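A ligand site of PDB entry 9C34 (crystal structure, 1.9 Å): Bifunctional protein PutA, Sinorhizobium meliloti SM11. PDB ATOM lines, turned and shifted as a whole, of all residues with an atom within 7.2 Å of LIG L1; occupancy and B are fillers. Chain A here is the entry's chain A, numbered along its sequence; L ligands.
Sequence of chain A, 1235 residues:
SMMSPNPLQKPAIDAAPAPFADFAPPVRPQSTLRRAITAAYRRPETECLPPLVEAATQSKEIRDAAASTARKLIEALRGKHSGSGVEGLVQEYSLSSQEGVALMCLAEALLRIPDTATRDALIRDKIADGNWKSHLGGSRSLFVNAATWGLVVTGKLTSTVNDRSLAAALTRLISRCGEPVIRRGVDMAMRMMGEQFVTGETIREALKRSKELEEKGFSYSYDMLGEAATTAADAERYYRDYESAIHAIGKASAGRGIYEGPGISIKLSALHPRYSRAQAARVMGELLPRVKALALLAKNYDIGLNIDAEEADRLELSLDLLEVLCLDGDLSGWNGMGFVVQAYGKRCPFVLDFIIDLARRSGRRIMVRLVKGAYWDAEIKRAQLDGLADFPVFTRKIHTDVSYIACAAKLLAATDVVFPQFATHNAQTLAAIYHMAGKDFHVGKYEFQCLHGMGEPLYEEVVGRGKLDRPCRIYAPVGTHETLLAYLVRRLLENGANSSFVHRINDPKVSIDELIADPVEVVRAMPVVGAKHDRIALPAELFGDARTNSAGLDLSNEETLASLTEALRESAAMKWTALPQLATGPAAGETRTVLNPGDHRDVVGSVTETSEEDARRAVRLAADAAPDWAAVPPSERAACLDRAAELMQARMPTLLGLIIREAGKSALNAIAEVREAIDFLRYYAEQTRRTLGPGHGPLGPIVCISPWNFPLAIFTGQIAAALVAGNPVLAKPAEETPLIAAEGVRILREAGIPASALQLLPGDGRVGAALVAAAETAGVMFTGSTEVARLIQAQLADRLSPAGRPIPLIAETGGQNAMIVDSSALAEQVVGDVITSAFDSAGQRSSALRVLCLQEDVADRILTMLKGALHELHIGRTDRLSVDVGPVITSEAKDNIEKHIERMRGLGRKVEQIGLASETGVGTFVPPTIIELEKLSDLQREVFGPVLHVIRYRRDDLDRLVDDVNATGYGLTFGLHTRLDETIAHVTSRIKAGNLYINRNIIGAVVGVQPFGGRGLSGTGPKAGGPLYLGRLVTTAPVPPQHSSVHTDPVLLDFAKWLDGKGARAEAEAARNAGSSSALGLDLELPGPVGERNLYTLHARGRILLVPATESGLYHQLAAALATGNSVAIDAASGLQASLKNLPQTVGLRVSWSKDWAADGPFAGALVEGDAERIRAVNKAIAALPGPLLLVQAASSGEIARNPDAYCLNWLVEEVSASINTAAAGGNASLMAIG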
ATOM      1  N   PHE A 197      21.610   0.733 -20.066  1.00  0.00           N
ATOM      2  CA  PHE A 197      20.946   0.579 -18.789  1.00  0.00           C
ATOM      3  C   PHE A 197      20.652  -0.866 -18.465  1.00  0.00           C
ATOM      4  O   PHE A 197      20.463  -1.196 -17.293  1.00  0.00           O
ATOM      5  CB  PHE A 197      19.623   1.348 -18.798  1.00  0.00           C
ATOM      6  CG  PHE A 197      19.815   2.839 -18.931  1.00  0.00           C
ATOM      7  CD1 PHE A 197      20.889   3.474 -18.336  1.00  0.00           C
ATOM      8  CD2 PHE A 197      18.926   3.598 -19.677  1.00  0.00           C
ATOM      9  CE1 PHE A 197      21.064   4.828 -18.451  1.00  0.00           C
ATOM     10  CE2 PHE A 197      19.100   4.973 -19.800  1.00  0.00           C
ATOM     11  CZ  PHE A 197      20.170   5.577 -19.183  1.00  0.00           C
ATOM     12  N   VAL A 198      20.596  -1.705 -19.481  1.00  0.00           N
ATOM     13  CA  VAL A 198      20.495  -3.147 -19.327  1.00  0.00           C
ATOM     14  C   VAL A 198      21.553  -3.798 -20.196  1.00  0.00           C
ATOM     15  O   VAL A 198      22.014  -3.256 -21.205  1.00  0.00           O
ATOM     16  CB  VAL A 198      19.086  -3.672 -19.698  1.00  0.00           C
ATOM     17  CG1 VAL A 198      18.069  -3.083 -18.770  1.00  0.00           C
ATOM     18  CG2 VAL A 198      18.765  -3.345 -21.141  1.00  0.00           C
ATOM     19  N   ASP A 223      20.776  -9.641 -13.031  1.00  0.00           N
ATOM     20  CA  ASP A 223      19.679  -9.141 -12.204  1.00  0.00           C
ATOM     21  C   ASP A 223      18.430  -8.935 -13.044  1.00  0.00           C
ATOM     22  O   ASP A 223      18.391  -8.025 -13.896  1.00  0.00           O
ATOM     23  CB  ASP A 223      20.084  -7.836 -11.524  1.00  0.00           C
ATOM     24  CG  ASP A 223      18.879  -7.100 -10.922  1.00  0.00           C
ATOM     25  OD1 ASP A 223      17.858  -7.762 -10.603  1.00  0.00           O
ATOM     26  OD2 ASP A 223      18.972  -5.860 -10.817  1.00  0.00           O
ATOM     27  N   LEU A 225      15.650  -7.595 -12.353  1.00  0.00           N
ATOM     28  CA  LEU A 225      14.938  -6.329 -12.132  1.00  0.00           C
ATOM     29  C   LEU A 225      13.556  -6.528 -11.499  1.00  0.00           C
ATOM     30  O   LEU A 225      12.719  -5.633 -11.554  1.00  0.00           O
ATOM     31  CB  LEU A 225      14.820  -5.532 -13.439  1.00  0.00           C
ATOM     32  CG  LEU A 225      16.093  -4.840 -13.977  1.00  0.00           C
ATOM     33  CD1 LEU A 225      15.818  -4.014 -15.231  1.00  0.00           C
ATOM     34  CD2 LEU A 225      16.810  -3.979 -12.935  1.00  0.00           C
ATOM     35  N   GLU A 227      11.288  -6.532  -8.130  1.00  0.00           N
ATOM     36  CA  GLU A 227      11.243  -6.164  -6.719  1.00  0.00           C
ATOM     37  C   GLU A 227       9.843  -5.715  -6.332  1.00  0.00           C
ATOM     38  O   GLU A 227       9.004  -5.427  -7.186  1.00  0.00           O
ATOM     39  CB  GLU A 227      12.258  -5.068  -6.377  1.00  0.00           C
ATOM     40  CG  GLU A 227      12.159  -3.794  -7.188  1.00  0.00           C
ATOM     41  CD  GLU A 227      13.260  -2.814  -6.829  1.00  0.00           C
ATOM     42  OE1 GLU A 227      13.380  -2.487  -5.627  1.00  0.00           O
ATOM     43  OE2 GLU A 227      14.023  -2.409  -7.733  1.00  0.00           O
ATOM     44  N   LYS A 267      16.069 -10.533  -5.380  1.00  0.00           N
ATOM     45  CA  LYS A 267      15.587  -9.690  -4.287  1.00  0.00           C
ATOM     46  C   LYS A 267      14.457 -10.444  -3.597  1.00  0.00           C
ATOM     47  O   LYS A 267      13.497 -10.853  -4.249  1.00  0.00           O
ATOM     48  CB  LYS A 267      15.079  -8.343  -4.800  1.00  0.00           C
ATOM     49  CG  LYS A 267      16.224  -7.371  -5.196  1.00  0.00           C
ATOM     50  CD  LYS A 267      15.682  -5.996  -5.594  1.00  0.00           C
ATOM     51  CE  LYS A 267      16.783  -4.926  -5.580  1.00  0.00           C
ATOM     52  NZ  LYS A 267      17.959  -5.240  -6.451  1.00  0.00           N
ATOM     53  N   LEU A 451      28.883  -2.415 -11.765  1.00  0.00           N
ATOM     54  CA  LEU A 451      27.594  -2.397 -12.440  1.00  0.00           C
ATOM     55  C   LEU A 451      27.826  -2.252 -13.936  1.00  0.00           C
ATOM     56  O   LEU A 451      28.691  -1.492 -14.367  1.00  0.00           O
ATOM     57  CB  LEU A 451      26.721  -1.253 -11.938  1.00  0.00           C
ATOM     58  CG  LEU A 451      26.201  -1.336 -10.485  1.00  0.00           C
ATOM     59  CD1 LEU A 451      25.330  -0.116 -10.183  1.00  0.00           C
ATOM     60  CD2 LEU A 451      25.387  -2.587 -10.153  1.00  0.00           C
ATOM     61  N   HIS A 452      27.046  -2.996 -14.727  1.00  0.00           N
ATOM     62  CA  HIS A 452      27.116  -2.881 -16.191  1.00  0.00           C
ATOM     63  C   HIS A 452      26.922  -1.421 -16.629  1.00  0.00           C
ATOM     64  O   HIS A 452      26.102  -0.695 -16.083  1.00  0.00           O
ATOM     65  CB  HIS A 452      26.045  -3.774 -16.849  1.00  0.00           C
ATOM     66  CG  HIS A 452      25.847  -3.493 -18.308  1.00  0.00           C
ATOM     67  ND1 HIS A 452      26.612  -4.091 -19.293  1.00  0.00           N
ATOM     68  CD2 HIS A 452      24.964  -2.699 -18.950  1.00  0.00           C
ATOM     69  CE1 HIS A 452      26.218  -3.647 -20.475  1.00  0.00           C
ATOM     70  NE2 HIS A 452      25.218  -2.798 -20.298  1.00  0.00           N
ATOM     71  N   TYR A 475      27.565  -6.832 -12.583  1.00  0.00           N
ATOM     72  CA  TYR A 475      26.145  -6.964 -12.236  1.00  0.00           C
ATOM     73  C   TYR A 475      25.311  -6.437 -13.405  1.00  0.00           C
ATOM     74  O   TYR A 475      25.400  -5.261 -13.769  1.00  0.00           O
ATOM     75  CB  TYR A 475      25.867  -6.200 -10.937  1.00  0.00           C
ATOM     76  CG  TYR A 475      24.484  -6.322 -10.355  1.00  0.00           C
ATOM     77  CD1 TYR A 475      23.480  -5.426 -10.732  1.00  0.00           C
ATOM     78  CD2 TYR A 475      24.185  -7.296  -9.396  1.00  0.00           C
ATOM     79  CE1 TYR A 475      22.194  -5.536 -10.223  1.00  0.00           C
ATOM     80  CE2 TYR A 475      22.887  -7.393  -8.839  1.00  0.00           C
ATOM     81  CZ  TYR A 475      21.906  -6.485  -9.251  1.00  0.00           C
ATOM     82  OH  TYR A 475      20.601  -6.538  -8.754  1.00  0.00           O
ATOM     83  N   ALA A 476      24.556  -7.319 -14.034  1.00  0.00           N
ATOM     84  CA  ALA A 476      24.014  -7.090 -15.380  1.00  0.00           C
ATOM     85  C   ALA A 476      22.490  -7.072 -15.321  1.00  0.00           C
ATOM     86  O   ALA A 476      21.865  -8.139 -15.250  1.00  0.00           O
ATOM     87  CB  ALA A 476      24.510  -8.187 -16.334  1.00  0.00           C
ATOM     88  N   PRO A 477      21.869  -5.896 -15.382  1.00  0.00           N
ATOM     89  CA  PRO A 477      20.408  -5.852 -15.350  1.00  0.00           C
ATOM     90  C   PRO A 477      19.860  -6.366 -16.672  1.00  0.00           C
ATOM     91  O   PRO A 477      20.462  -6.194 -17.735  1.00  0.00           O
ATOM     92  CB  PRO A 477      20.077  -4.369 -15.164  1.00  0.00           C
ATOM     93  CG  PRO A 477      21.332  -3.720 -14.872  1.00  0.00           C
ATOM     94  CD  PRO A 477      22.449  -4.559 -15.419  1.00  0.00           C
ATOM     95  N   THR A 483      10.382  -2.226 -17.584  1.00  0.00           N
ATOM     96  CA  THR A 483      10.971  -2.748 -16.359  1.00  0.00           C
ATOM     97  C   THR A 483      12.143  -1.880 -15.899  1.00  0.00           C
ATOM     98  O   THR A 483      12.255  -1.564 -14.714  1.00  0.00           O
ATOM     99  CB  THR A 483      11.418  -4.200 -16.570  1.00  0.00           C
ATOM    100  OG1 THR A 483      10.328  -4.989 -17.044  1.00  0.00           O
ATOM    101  CG2 THR A 483      11.907  -4.773 -15.269  1.00  0.00           C
ATOM    102  N   LEU A 484      13.034  -1.509 -16.824  1.00  0.00           N
ATOM    103  CA  LEU A 484      14.235  -0.775 -16.429  1.00  0.00           C
ATOM    104  C   LEU A 484      13.863   0.522 -15.724  1.00  0.00           C
ATOM    105  O   LEU A 484      14.439   0.869 -14.691  1.00  0.00           O
ATOM    106  CB  LEU A 484      15.123  -0.494 -17.652  1.00  0.00           C
ATOM    107  N   LEU A 485      12.840   1.221 -16.253  1.00  0.00           N
ATOM    108  CA  LEU A 485      12.492   2.565 -15.790  1.00  0.00           C
ATOM    109  C   LEU A 485      11.842   2.586 -14.408  1.00  0.00           C
ATOM    110  O   LEU A 485      11.786   3.649 -13.786  1.00  0.00           O
ATOM    111  CB  LEU A 485      11.536   3.234 -16.807  1.00  0.00           C
ATOM    112  CG  LEU A 485      12.089   3.415 -18.219  1.00  0.00           C
ATOM    113  CD1 LEU A 485      10.987   3.422 -19.264  1.00  0.00           C
ATOM    114  CD2 LEU A 485      12.887   4.689 -18.325  1.00  0.00           C
ATOM    115  N   ALA A 486      11.329   1.444 -13.936  1.00  0.00           N
ATOM    116  CA  ALA A 486      10.711   1.409 -12.615  1.00  0.00           C
ATOM    117  C   ALA A 486      11.677   1.871 -11.522  1.00  0.00           C
ATOM    118  O   ALA A 486      11.265   2.507 -10.549  1.00  0.00           O
ATOM    119  CB  ALA A 486      10.204   0.002 -12.289  1.00  0.00           C
ATOM    120  N   TYR A 487      12.972   1.571 -11.673  1.00  0.00           N
ATOM    121  CA  TYR A 487      13.937   1.913 -10.631  1.00  0.00           C
ATOM    122  C   TYR A 487      15.280   2.325 -11.229  1.00  0.00           C
ATOM    123  O   TYR A 487      16.329   2.126 -10.598  1.00  0.00           O
ATOM    124  CB  TYR A 487      14.163   0.740  -9.667  1.00  0.00           C
ATOM    125  N   LEU A 488      15.285   2.889 -12.439  1.00  0.00           N
ATOM    126  CA  LEU A 488      16.516   3.441 -12.991  1.00  0.00           C
ATOM    127  C   LEU A 488      16.952   4.681 -12.241  1.00  0.00           C
ATOM    128  O   LEU A 488      18.133   5.045 -12.265  1.00  0.00           O
ATOM    129  CB  LEU A 488      16.353   3.778 -14.481  1.00  0.00           C
ATOM    130  N   VAL A 489      15.998   5.366 -11.581  1.00  0.00           N
ATOM    131  CA  VAL A 489      16.338   6.570 -10.846  1.00  0.00           C
ATOM    132  C   VAL A 489      17.216   6.223  -9.657  1.00  0.00           C
ATOM    133  O   VAL A 489      18.230   6.883  -9.418  1.00  0.00           O
ATOM    134  CB  VAL A 489      15.069   7.307 -10.389  1.00  0.00           C
ATOM    135  CG1 VAL A 489      15.463   8.457  -9.447  1.00  0.00           C
ATOM    136  CG2 VAL A 489      14.289   7.834 -11.575  1.00  0.00           C
ATOM    137  N   ARG A 490      16.799   5.240  -8.852  1.00  0.00           N
ATOM    138  CA  ARG A 490      17.592   4.834  -7.689  1.00  0.00           C
ATOM    139  C   ARG A 490      19.011   4.508  -8.131  1.00  0.00           C
ATOM    140  O   ARG A 490      19.981   4.862  -7.448  1.00  0.00           O
ATOM    141  CB  ARG A 490      16.962   3.628  -6.976  1.00  0.00           C
ATOM    142  CG  ARG A 490      17.766   3.125  -5.765  1.00  0.00           C
ATOM    143  CD  ARG A 490      17.143   1.897  -5.086  1.00  0.00           C
ATOM    144  NE  ARG A 490      17.252   0.704  -5.913  1.00  0.00           N
ATOM    145  CZ  ARG A 490      16.227  -0.058  -6.295  1.00  0.00           C
ATOM    146  NH1 ARG A 490      14.988   0.179  -5.871  1.00  0.00           N
ATOM    147  NH2 ARG A 490      16.452  -1.082  -7.113  1.00  0.00           N
ATOM    148  N   ARG A 491      19.150   3.910  -9.310  1.00  0.00           N
ATOM    149  CA  ARG A 491      20.450   3.495  -9.801  1.00  0.00           C
ATOM    150  C   ARG A 491      21.262   4.656 -10.345  1.00  0.00           C
ATOM    151  O   ARG A 491      22.492   4.623 -10.269  1.00  0.00           O
ATOM    152  CB  ARG A 491      20.306   2.436 -10.900  1.00  0.00           C
ATOM    153  CG  ARG A 491      21.591   2.176 -11.676  1.00  0.00           C
ATOM    154  CD  ARG A 491      22.771   1.623 -10.838  1.00  0.00           C
ATOM    155  NE  ARG A 491      22.679   1.807  -9.392  1.00  0.00           N
ATOM    156  CZ  ARG A 491      22.022   0.980  -8.589  1.00  0.00           C
ATOM    157  NH1 ARG A 491      21.387  -0.074  -9.059  1.00  0.00           N
ATOM    158  NH2 ARG A 491      21.968   1.251  -7.281  1.00  0.00           N
ATOM    159  N   LEU A 492      20.621   5.655 -10.919  1.00  0.00           N
ATOM    160  CA  LEU A 492      21.351   6.856 -11.312  1.00  0.00           C
ATOM    161  C   LEU A 492      21.660   7.716 -10.095  1.00  0.00           C
ATOM    162  O   LEU A 492      22.829   7.966  -9.787  1.00  0.00           O
ATOM    163  CB  LEU A 492      20.560   7.660 -12.347  1.00  0.00           C
ATOM    164  CG  LEU A 492      20.519   7.170 -13.783  1.00  0.00           C
ATOM    165  CD1 LEU A 492      19.315   7.838 -14.430  1.00  0.00           C
ATOM    166  CD2 LEU A 492      21.772   7.490 -14.567  1.00  0.00           C
HETATM  167  N1  LIG L   1      19.059  -1.649 -10.789  1.00  0.00           N
HETATM  168  C1  LIG L   1      18.793  -0.465 -11.760  1.00  0.00           C
HETATM  169  C2  LIG L   1      17.219  -0.502 -12.145  1.00  0.00           C
HETATM  170  O1  LIG L   1      16.493  -0.954 -11.231  1.00  0.00           O
HETATM  171  C3  LIG L   1      19.769  -0.686 -12.926  1.00  0.00           C
HETATM  172  C4  LIG L   1      20.954  -1.459 -12.326  1.00  0.00           C
HETATM  173  C5  LIG L   1      20.385  -2.316 -11.215  1.00  0.00           C
HETATM  174  O2  LIG L   1      16.942  -0.034 -13.284  1.00  0.00           O
HETATM  175  C1  LG2 L   2      19.761  -1.781  -6.736  1.00  0.00           C
HETATM  176  N1  LG2 L   2      20.851  -3.786  -5.696  1.00  0.00           N
HETATM  177  O1  LG2 L   2      18.925  -2.557  -7.293  1.00  0.00           O
HETATM  178  C2  LG2 L   2      21.041  -2.355  -6.086  1.00  0.00           C
HETATM  179  C3  LG2 L   2      22.254  -2.391  -7.049  1.00  0.00           C
HETATM  180  C4  LG2 L   2      22.293  -3.844  -7.524  1.00  0.00           C
HETATM  181  C5  LG2 L   2      21.492  -4.609  -6.519  1.00  0.00           C
HETATM  182  O2  LG2 L   2      19.684  -0.545  -6.641  1.00  0.00           O
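The backbone carbonyl oxygen (O) of Leu 484 lies close to an oxygen (O2) of LIG L1.
The guanidinium group (NH1) of Arg 491 sits close to a nitrogen (N1) of LIG L1 (3.3 Å).
An oxygen (O2) of LIG L1 sits at hydrogen-bond distance from the backbone NH of Leu 488 (3.5 Å).
The guanidinium group (NH2) of Arg 491 lies within salt-bridge range of an oxygen (O2) of LG2 L2 (3.0 Å).
NE of Arg 490 lies within salt-bridge range of O2 of LG2 L2, at 2.8 Å.
The side-chain amino group (NZ) of Lys 267 is in salt-bridge range of an oxygen (O1) of LG2 L2, at 3.0 Å.
The backbone NH of Leu 225 lies within hydrogen-bond range of the side-chain carboxylate of Asp 223 (2.8 Å).
OH of Tyr 475 sits at hydrogen-bond distance from OD2 of Asp 223.
N of His 452 is in hydrogen-bond range of O of Tyr 475, 3.0 Å away.
The backbone NH (N) of Asp 223 lies within hydrogen-bond range of the backbone carbonyl oxygen (O) of Ala 476, 2.9 Å away.
O of Tyr 487 sits close to O1 of LIG L1 (3.1 Å).
Asp 223 touches LIG L1 (OD2 to C5, 3.8 Å).
Leu 225 touches LIG L1.
Tyr 475 touches LIG L1 (CE1 to C5, 3.8 Å).
CG of Pro 477 touches C4 of LIG L1 (3.4 Å).
Within 4 Å of LIG L1: Asp 223, Leu 225, Tyr 475, Pro 477, Leu 484, Tyr 487, Leu 488 and Arg 491.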
